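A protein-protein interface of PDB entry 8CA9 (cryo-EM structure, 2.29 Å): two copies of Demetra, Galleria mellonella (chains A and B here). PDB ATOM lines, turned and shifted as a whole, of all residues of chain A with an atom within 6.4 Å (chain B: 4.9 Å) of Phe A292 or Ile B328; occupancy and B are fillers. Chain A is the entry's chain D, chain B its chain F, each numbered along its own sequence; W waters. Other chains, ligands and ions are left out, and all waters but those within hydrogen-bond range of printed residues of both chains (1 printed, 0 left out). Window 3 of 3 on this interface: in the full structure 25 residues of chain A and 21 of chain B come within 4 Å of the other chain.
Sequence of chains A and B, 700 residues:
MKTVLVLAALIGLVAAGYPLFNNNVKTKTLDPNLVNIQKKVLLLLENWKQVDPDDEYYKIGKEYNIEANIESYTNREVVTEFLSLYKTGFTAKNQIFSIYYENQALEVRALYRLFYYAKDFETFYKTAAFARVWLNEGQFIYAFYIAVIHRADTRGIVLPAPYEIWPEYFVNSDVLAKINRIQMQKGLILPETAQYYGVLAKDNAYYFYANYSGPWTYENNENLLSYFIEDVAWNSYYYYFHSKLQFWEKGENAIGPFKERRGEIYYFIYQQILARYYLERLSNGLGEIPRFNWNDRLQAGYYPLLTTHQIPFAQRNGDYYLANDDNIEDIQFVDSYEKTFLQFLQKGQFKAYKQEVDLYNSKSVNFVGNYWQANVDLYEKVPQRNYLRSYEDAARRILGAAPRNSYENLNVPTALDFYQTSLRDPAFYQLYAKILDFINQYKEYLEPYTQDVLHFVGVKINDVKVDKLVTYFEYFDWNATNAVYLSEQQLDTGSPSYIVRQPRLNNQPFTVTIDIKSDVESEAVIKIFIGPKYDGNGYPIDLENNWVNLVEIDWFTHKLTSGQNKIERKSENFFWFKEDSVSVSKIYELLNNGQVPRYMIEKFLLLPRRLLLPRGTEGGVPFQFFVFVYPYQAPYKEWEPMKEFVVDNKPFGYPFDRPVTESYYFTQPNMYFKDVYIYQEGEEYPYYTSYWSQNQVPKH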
ATOM      1  N   PRO A 290      22.975  -1.527  -6.315  1.00  0.00           N
ATOM      2  CA  PRO A 290      22.340  -2.223  -5.190  1.00  0.00           C
ATOM      3  C   PRO A 290      22.477  -3.734  -5.291  1.00  0.00           C
ATOM      4  O   PRO A 290      22.539  -4.311  -6.380  1.00  0.00           O
ATOM      5  CB  PRO A 290      20.869  -1.798  -5.289  1.00  0.00           C
ATOM      6  CG  PRO A 290      20.870  -0.571  -6.121  1.00  0.00           C
ATOM      7  CD  PRO A 290      22.000  -0.732  -7.079  1.00  0.00           C
ATOM      8  N   ARG A 291      22.520  -4.374  -4.126  1.00  0.00           N
ATOM      9  CA  ARG A 291      22.464  -5.823  -4.006  1.00  0.00           C
ATOM     10  C   ARG A 291      21.085  -6.246  -3.509  1.00  0.00           C
ATOM     11  O   ARG A 291      20.380  -5.485  -2.842  1.00  0.00           O
ATOM     12  CB  ARG A 291      23.548  -6.337  -3.055  1.00  0.00           C
ATOM     13  CG  ARG A 291      24.897  -6.591  -3.720  1.00  0.00           C
ATOM     14  CD  ARG A 291      25.495  -5.326  -4.315  1.00  0.00           C
ATOM     15  NE  ARG A 291      26.796  -5.574  -4.924  1.00  0.00           N
ATOM     16  CZ  ARG A 291      27.539  -4.646  -5.514  1.00  0.00           C
ATOM     17  NH1 ARG A 291      27.133  -3.390  -5.606  1.00  0.00           N
ATOM     18  NH2 ARG A 291      28.719  -4.987  -6.023  1.00  0.00           N
ATOM     19  N   PHE A 292      20.707  -7.478  -3.842  1.00  0.00           N
ATOM     20  CA  PHE A 292      19.371  -7.966  -3.533  1.00  0.00           C
ATOM     21  C   PHE A 292      19.447  -9.409  -3.061  1.00  0.00           C
ATOM     22  O   PHE A 292      20.444 -10.105  -3.270  1.00  0.00           O
ATOM     23  CB  PHE A 292      18.438  -7.856  -4.746  1.00  0.00           C
ATOM     24  CG  PHE A 292      18.780  -8.801  -5.862  1.00  0.00           C
ATOM     25  CD1 PHE A 292      19.751  -8.474  -6.792  1.00  0.00           C
ATOM     26  CD2 PHE A 292      18.124 -10.014  -5.985  1.00  0.00           C
ATOM     27  CE1 PHE A 292      20.066  -9.341  -7.820  1.00  0.00           C
ATOM     28  CE2 PHE A 292      18.435 -10.885  -7.010  1.00  0.00           C
ATOM     29  CZ  PHE A 292      19.406 -10.547  -7.929  1.00  0.00           C
ATOM     30  N   ASN A 293      18.369  -9.847  -2.414  1.00  0.00           N
ATOM     31  CA  ASN A 293      18.235 -11.204  -1.901  1.00  0.00           C
ATOM     32  C   ASN A 293      17.106 -11.902  -2.645  1.00  0.00           C
ATOM     33  O   ASN A 293      16.029 -11.324  -2.826  1.00  0.00           O
ATOM     34  CB  ASN A 293      17.956 -11.195  -0.395  1.00  0.00           C
ATOM     35  CG  ASN A 293      17.769 -12.587   0.172  1.00  0.00           C
ATOM     36  OD1 ASN A 293      18.116 -13.583  -0.463  1.00  0.00           O
ATOM     37  ND2 ASN A 293      17.221 -12.664   1.379  1.00  0.00           N
ATOM     38  N   TRP A 294      17.353 -13.141  -3.073  1.00  0.00           N
ATOM     39  CA  TRP A 294      16.347 -13.866  -3.841  1.00  0.00           C
ATOM     40  C   TRP A 294      15.081 -14.094  -3.025  1.00  0.00           C
ATOM     41  O   TRP A 294      13.967 -13.939  -3.539  1.00  0.00           O
ATOM     42  CB  TRP A 294      16.912 -15.199  -4.326  1.00  0.00           C
ATOM     43  CG  TRP A 294      17.892 -15.057  -5.441  1.00  0.00           C
ATOM     44  CD1 TRP A 294      19.234 -15.293  -5.386  1.00  0.00           C
ATOM     45  CD2 TRP A 294      17.611 -14.639  -6.781  1.00  0.00           C
ATOM     46  NE1 TRP A 294      19.806 -15.052  -6.611  1.00  0.00           N
ATOM     47  CE2 TRP A 294      18.831 -14.648  -7.484  1.00  0.00           C
ATOM     48  CE3 TRP A 294      16.447 -14.259  -7.456  1.00  0.00           C
ATOM     49  CZ2 TRP A 294      18.921 -14.293  -8.828  1.00  0.00           C
ATOM     50  CZ3 TRP A 294      16.538 -13.907  -8.789  1.00  0.00           C
ATOM     51  CH2 TRP A 294      17.765 -13.926  -9.461  1.00  0.00           C
ATOM     52  N   ASP A 296      14.029 -12.228  -0.757  1.00  0.00           N
ATOM     53  CA  ASP A 296      13.429 -10.919  -0.563  1.00  0.00           C
ATOM     54  C   ASP A 296      12.989 -10.377  -1.920  1.00  0.00           C
ATOM     55  O   ASP A 296      13.084 -11.058  -2.945  1.00  0.00           O
ATOM     56  CB  ASP A 296      14.409  -9.967   0.130  1.00  0.00           C
ATOM     57  CG  ASP A 296      13.706  -8.845   0.871  1.00  0.00           C
ATOM     58  OD1 ASP A 296      12.963  -9.141   1.829  1.00  0.00           O
ATOM     59  OD2 ASP A 296      13.896  -7.669   0.496  1.00  0.00           O
ATOM     60  N   ARG A 297      12.502  -9.142  -1.927  1.00  0.00           N
ATOM     61  CA  ARG A 297      11.930  -8.536  -3.120  1.00  0.00           C
ATOM     62  C   ARG A 297      12.907  -7.564  -3.773  1.00  0.00           C
ATOM     63  O   ARG A 297      13.676  -6.873  -3.101  1.00  0.00           O
ATOM     64  CB  ARG A 297      10.625  -7.812  -2.779  1.00  0.00           C
ATOM     65  CG  ARG A 297      10.676  -6.975  -1.511  1.00  0.00           C
ATOM     66  CD  ARG A 297       9.387  -6.195  -1.306  1.00  0.00           C
ATOM     67  NE  ARG A 297       8.204  -7.015  -1.548  1.00  0.00           N
ATOM     68  CZ  ARG A 297       6.961  -6.554  -1.541  1.00  0.00           C
ATOM     69  NH1 ARG A 297       6.695  -5.282  -1.289  1.00  0.00           N
ATOM     70  NH2 ARG A 297       5.957  -7.389  -1.795  1.00  0.00           N
ATOM     71  N   LEU A 298      12.859  -7.522  -5.104  1.00  0.00           N
ATOM     72  CA  LEU A 298      13.674  -6.593  -5.876  1.00  0.00           C
ATOM     73  C   LEU A 298      13.118  -5.183  -5.742  1.00  0.00           C
ATOM     74  O   LEU A 298      11.902  -4.981  -5.689  1.00  0.00           O
ATOM     75  CB  LEU A 298      13.711  -7.010  -7.348  1.00  0.00           C
ATOM     76  CG  LEU A 298      14.629  -6.215  -8.280  1.00  0.00           C
ATOM     77  CD1 LEU A 298      16.095  -6.426  -7.928  1.00  0.00           C
ATOM     78  CD2 LEU A 298      14.371  -6.598  -9.726  1.00  0.00           C
ATOM     79  N   GLN A 299      14.018  -4.205  -5.683  1.00  0.00           N
ATOM     80  CA  GLN A 299      13.667  -2.811  -5.446  1.00  0.00           C
ATOM     81  C   GLN A 299      14.062  -1.933  -6.628  1.00  0.00           C
ATOM     82  O   GLN A 299      14.630  -0.852  -6.462  1.00  0.00           O
ATOM     83  CB  GLN A 299      14.316  -2.309  -4.159  1.00  0.00           C
ATOM     84  CG  GLN A 299      13.863  -3.058  -2.915  1.00  0.00           C
ATOM     85  CD  GLN A 299      14.839  -2.925  -1.766  1.00  0.00           C
ATOM     86  OE1 GLN A 299      15.037  -1.838  -1.225  1.00  0.00           O
ATOM     87  NE2 GLN A 299      15.462  -4.036  -1.389  1.00  0.00           N
ATOM     88  N   LEU A 322      10.189 -11.744  -5.596  1.00  0.00           N
ATOM     89  CA  LEU A 322      10.705 -12.673  -6.595  1.00  0.00           C
ATOM     90  C   LEU A 322      10.234 -14.104  -6.373  1.00  0.00           C
ATOM     91  O   LEU A 322      10.126 -14.862  -7.343  1.00  0.00           O
ATOM     92  CB  LEU A 322      12.234 -12.631  -6.593  1.00  0.00           C
ATOM     93  CG  LEU A 322      12.851 -11.260  -6.884  1.00  0.00           C
ATOM     94  CD1 LEU A 322      14.327 -11.248  -6.528  1.00  0.00           C
ATOM     95  CD2 LEU A 322      12.648 -10.879  -8.340  1.00  0.00           C
ATOM     96  N   LEU A 399      13.571 -12.462 -12.899  1.00  0.00           N
ATOM     97  CA  LEU A 399      13.632 -11.007 -12.833  1.00  0.00           C
ATOM     98  C   LEU A 399      12.740 -10.324 -13.861  1.00  0.00           C
ATOM     99  O   LEU A 399      12.394  -9.152 -13.675  1.00  0.00           O
ATOM    100  CB  LEU A 399      15.078 -10.539 -13.023  1.00  0.00           C
ATOM    101  CG  LEU A 399      16.067 -10.956 -11.931  1.00  0.00           C
ATOM    102  CD1 LEU A 399      17.498 -10.701 -12.379  1.00  0.00           C
ATOM    103  CD2 LEU A 399      15.777 -10.226 -10.630  1.00  0.00           C
ATOM    104  N   ALA A 427      18.060  -4.586 -13.463  1.00  0.00           N
ATOM    105  CA  ALA A 427      18.186  -5.926 -12.901  1.00  0.00           C
ATOM    106  C   ALA A 427      19.332  -6.693 -13.545  1.00  0.00           C
ATOM    107  O   ALA A 427      19.986  -7.503 -12.882  1.00  0.00           O
ATOM    108  CB  ALA A 427      16.872  -6.689 -13.068  1.00  0.00           C
ATOM    109  N   GLN A 430      22.419  -5.554 -11.695  1.00  0.00           N
ATOM    110  CA  GLN A 430      22.452  -6.109 -10.342  1.00  0.00           C
ATOM    111  C   GLN A 430      22.825  -7.591 -10.358  1.00  0.00           C
ATOM    112  O   GLN A 430      23.672  -8.046  -9.576  1.00  0.00           O
ATOM    113  CB  GLN A 430      21.099  -5.899  -9.662  1.00  0.00           C
ATOM    114  CG  GLN A 430      20.716  -4.438  -9.488  1.00  0.00           C
ATOM    115  CD  GLN A 430      19.467  -4.253  -8.651  1.00  0.00           C
ATOM    116  OE1 GLN A 430      19.056  -5.152  -7.918  1.00  0.00           O
ATOM    117  NE2 GLN A 430      18.852  -3.080  -8.759  1.00  0.00           N
ATOM    118  N   LEU A 431      22.204  -8.360 -11.256  1.00  0.00           N
ATOM    119  CA  LEU A 431      22.472  -9.793 -11.332  1.00  0.00           C
ATOM    120  C   LEU A 431      23.932 -10.060 -11.672  1.00  0.00           C
ATOM    121  O   LEU A 431      24.596 -10.889 -11.032  1.00  0.00           O
ATOM    122  CB  LEU A 431      21.548 -10.429 -12.373  1.00  0.00           C
ATOM    123  CG  LEU A 431      21.812 -11.881 -12.778  1.00  0.00           C
ATOM    124  CD1 LEU A 431      21.581 -12.817 -11.606  1.00  0.00           C
ATOM    125  CD2 LEU A 431      20.936 -12.265 -13.962  1.00  0.00           C
ATOM    126  N   LYS A 434      26.229  -9.366  -8.821  1.00  0.00           N
ATOM    127  CA  LYS A 434      26.259 -10.509  -7.908  1.00  0.00           C
ATOM    128  C   LYS A 434      27.185 -11.605  -8.434  1.00  0.00           C
ATOM    129  O   LYS A 434      28.008 -12.166  -7.692  1.00  0.00           O
ATOM    130  CB  LYS A 434      24.838 -11.044  -7.713  1.00  0.00           C
ATOM    131  CG  LYS A 434      24.720 -12.285  -6.837  1.00  0.00           C
ATOM    132  CD  LYS A 434      23.353 -12.944  -6.990  1.00  0.00           C
ATOM    133  CE  LYS A 434      22.243 -12.122  -6.354  1.00  0.00           C
ATOM    134  NZ  LYS A 434      22.338 -12.104  -4.869  1.00  0.00           N
ATOM    135  N   ASN B 324      19.450  -8.238   5.490  1.00  0.00           N
ATOM    136  CA  ASN B 324      19.236  -6.969   4.813  1.00  0.00           C
ATOM    137  C   ASN B 324      20.109  -6.905   3.561  1.00  0.00           C
ATOM    138  O   ASN B 324      20.794  -7.865   3.197  1.00  0.00           O
ATOM    139  CB  ASN B 324      19.514  -5.799   5.761  1.00  0.00           C
ATOM    140  CG  ASN B 324      20.839  -5.933   6.483  1.00  0.00           C
ATOM    141  OD1 ASN B 324      21.376  -7.030   6.623  1.00  0.00           O
ATOM    142  ND2 ASN B 324      21.369  -4.811   6.955  1.00  0.00           N
ATOM    143  N   ASP B 325      20.073  -5.749   2.895  1.00  0.00           N
ATOM    144  CA  ASP B 325      20.749  -5.613   1.608  1.00  0.00           C
ATOM    145  C   ASP B 325      22.256  -5.811   1.741  1.00  0.00           C
ATOM    146  O   ASP B 325      22.885  -6.432   0.876  1.00  0.00           O
ATOM    147  CB  ASP B 325      20.439  -4.244   1.002  1.00  0.00           C
ATOM    148  CG  ASP B 325      18.951  -4.014   0.816  1.00  0.00           C
ATOM    149  OD1 ASP B 325      18.223  -4.996   0.563  1.00  0.00           O
ATOM    150  OD2 ASP B 325      18.510  -2.851   0.925  1.00  0.00           O
ATOM    151  N   ASP B 326      22.851  -5.292   2.813  1.00  0.00           N
ATOM    152  CA  ASP B 326      24.302  -5.282   2.957  1.00  0.00           C
ATOM    153  C   ASP B 326      24.864  -6.546   3.598  1.00  0.00           C
ATOM    154  O   ASP B 326      26.085  -6.633   3.776  1.00  0.00           O
ATOM    155  CB  ASP B 326      24.732  -4.062   3.779  1.00  0.00           C
ATOM    156  CG  ASP B 326      24.496  -2.754   3.048  1.00  0.00           C
ATOM    157  OD1 ASP B 326      24.652  -2.725   1.810  1.00  0.00           O
ATOM    158  OD2 ASP B 326      24.157  -1.753   3.714  1.00  0.00           O
ATOM    159  N   ASN B 327      24.025  -7.523   3.949  1.00  0.00           N
ATOM    160  CA  ASN B 327      24.487  -8.747   4.592  1.00  0.00           C
ATOM    161  C   ASN B 327      24.323 -10.000   3.745  1.00  0.00           C
ATOM    162  O   ASN B 327      24.830 -11.057   4.144  1.00  0.00           O
ATOM    163  CB  ASN B 327      23.748  -8.969   5.923  1.00  0.00           C
ATOM    164  CG  ASN B 327      24.216  -8.033   7.016  1.00  0.00           C
ATOM    165  OD1 ASN B 327      25.309  -7.471   6.948  1.00  0.00           O
ATOM    166  ND2 ASN B 327      23.392  -7.871   8.046  1.00  0.00           N
ATOM    167  N   ILE B 328      23.656  -9.917   2.589  1.00  0.00           N
ATOM    168  CA  ILE B 328      23.245 -11.125   1.870  1.00  0.00           C
ATOM    169  C   ILE B 328      24.406 -12.104   1.758  1.00  0.00           C
ATOM    170  O   ILE B 328      24.298 -13.269   2.161  1.00  0.00           O
ATOM    171  CB  ILE B 328      22.671 -10.762   0.486  1.00  0.00           C
ATOM    172  CG1 ILE B 328      22.160 -12.016  -0.231  1.00  0.00           C
ATOM    173  CG2 ILE B 328      23.708 -10.056  -0.382  1.00  0.00           C
ATOM    174  CD1 ILE B 328      21.049 -12.739   0.505  1.00  0.00           C
ATOM    175  N   GLU B 329      25.546 -11.636   1.245  1.00  0.00           N
ATOM    176  CA  GLU B 329      26.690 -12.520   1.053  1.00  0.00           C
ATOM    177  C   GLU B 329      26.970 -13.317   2.320  1.00  0.00           C
ATOM    178  O   GLU B 329      26.929 -14.553   2.318  1.00  0.00           O
ATOM    179  CB  GLU B 329      27.921 -11.710   0.642  1.00  0.00           C
ATOM    180  CG  GLU B 329      27.752 -10.930  -0.652  1.00  0.00           C
ATOM    181  CD  GLU B 329      29.055 -10.332  -1.145  1.00  0.00           C
ATOM    182  OE1 GLU B 329      30.122 -10.702  -0.610  1.00  0.00           O
ATOM    183  OE2 GLU B 329      29.013  -9.492  -2.069  1.00  0.00           O
ATOM    184  N   ASP B 330      27.210 -12.614   3.429  1.00  0.00           N
ATOM    185  CA  ASP B 330      27.484 -13.301   4.686  1.00  0.00           C
ATOM    186  C   ASP B 330      26.396 -14.321   4.986  1.00  0.00           C
ATOM    187  O   ASP B 330      26.684 -15.499   5.231  1.00  0.00           O
ATOM    188  CB  ASP B 330      27.604 -12.286   5.823  1.00  0.00           C
ATOM    189  CG  ASP B 330      28.862 -11.446   5.726  1.00  0.00           C
ATOM    190  OD1 ASP B 330      29.655 -11.662   4.785  1.00  0.00           O
ATOM    191  OD2 ASP B 330      29.061 -10.569   6.593  1.00  0.00           O
ATOM    192  N   ILE B 331      25.132 -13.894   4.916  1.00  0.00           N
ATOM    193  CA  ILE B 331      24.026 -14.814   5.164  1.00  0.00           C
ATOM    194  C   ILE B 331      24.227 -16.085   4.356  1.00  0.00           C
ATOM    195  O   ILE B 331      24.267 -17.195   4.903  1.00  0.00           O
ATOM    196  CB  ILE B 331      22.681 -14.144   4.831  1.00  0.00           C
ATOM    197  CG1 ILE B 331      22.375 -13.015   5.821  1.00  0.00           C
ATOM    198  CG2 ILE B 331      21.560 -15.173   4.822  1.00  0.00           C
ATOM    199  CD1 ILE B 331      22.023 -13.487   7.219  1.00  0.00           C
ATOM    200  N   GLN B 332      24.429 -15.932   3.045  1.00  0.00           N
ATOM    201  CA  GLN B 332      24.581 -17.097   2.184  1.00  0.00           C
ATOM    202  C   GLN B 332      25.636 -18.031   2.753  1.00  0.00           C
ATOM    203  O   GLN B 332      25.368 -19.213   3.007  1.00  0.00           O
ATOM    204  CB  GLN B 332      24.958 -16.655   0.769  1.00  0.00           C
ATOM    205  CG  GLN B 332      24.326 -17.481  -0.338  1.00  0.00           C
ATOM    206  CD  GLN B 332      22.870 -17.129  -0.569  1.00  0.00           C
ATOM    207  OE1 GLN B 332      22.304 -16.287   0.128  1.00  0.00           O
ATOM    208  NE2 GLN B 332      22.256 -17.771  -1.555  1.00  0.00           N
HETATM  209  O   HOH W   1      20.372 -14.681  -2.181  1.00  0.00           O
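No position is printed for both chains. Of the 4 pairs that touch across the chains among the printed residues, none has its exchanged pair printed and touching as well.
Among the printed residues, pairs that only touch across the chains: Arg A291 with Asp B325 (3.99 Å), Phe A292 with Ile B328 (3.98 Å), Asn A293 with Ile B328 (3.2 Å) and Gln A299 with Asp B325 (3.5 Å).
Of the 9 printed residues of chain B, 2 touch a printed residue of chain A. Hydrophobic or aromatic side chains of chain B within 4 Å of the printed part of chain A: Ile B328. Of the 15 printed residues of chain A, 4 touch a printed residue of chain B. Among the printed residues, no Asp or Glu carboxylate lies within 4 Å of a Lys or Arg side-chain nitrogen of the other chain.
Water W1 bridges the side-chain amide oxygen of Asn A293 (3.0 Å) and the side-chain amide oxygen of Gln B332 (3.4 Å).
Of the printed residues of chain B, Arg A291 touches Asp B325. Phe A292 touches one residue of chain B. Printed residues of chain B within 4 Å of Asn A293: Ile B328 (3.2 Å). Arg A297 touches none of the printed residues of chain B. Of the printed residues of chain B, Gln A299 touches Asp B325 (3.5 Å). Printed residues of chain A within 4 Å of Asp B325: Arg A291 and Gln A299. Of chain A, only Phe A292 and Asn A293 come within 4 Å of Ile B328. The nearest printed residue of chain B that does not touch Phe A292 is Asp B325 (5.2 Å). The nearest residue of chain A that does not touch Ile B328 is Arg A291 (4.6 Å). The nearest printed residue of chain A that does not touch Asp B325 is Asp A296 (5.1 Å).
The backbone carbonyl oxygen (O) of Phe A292 lies within hydrogen-bond range of the side-chain amino group (NZ) of Lys A434, 3.2 Å away.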
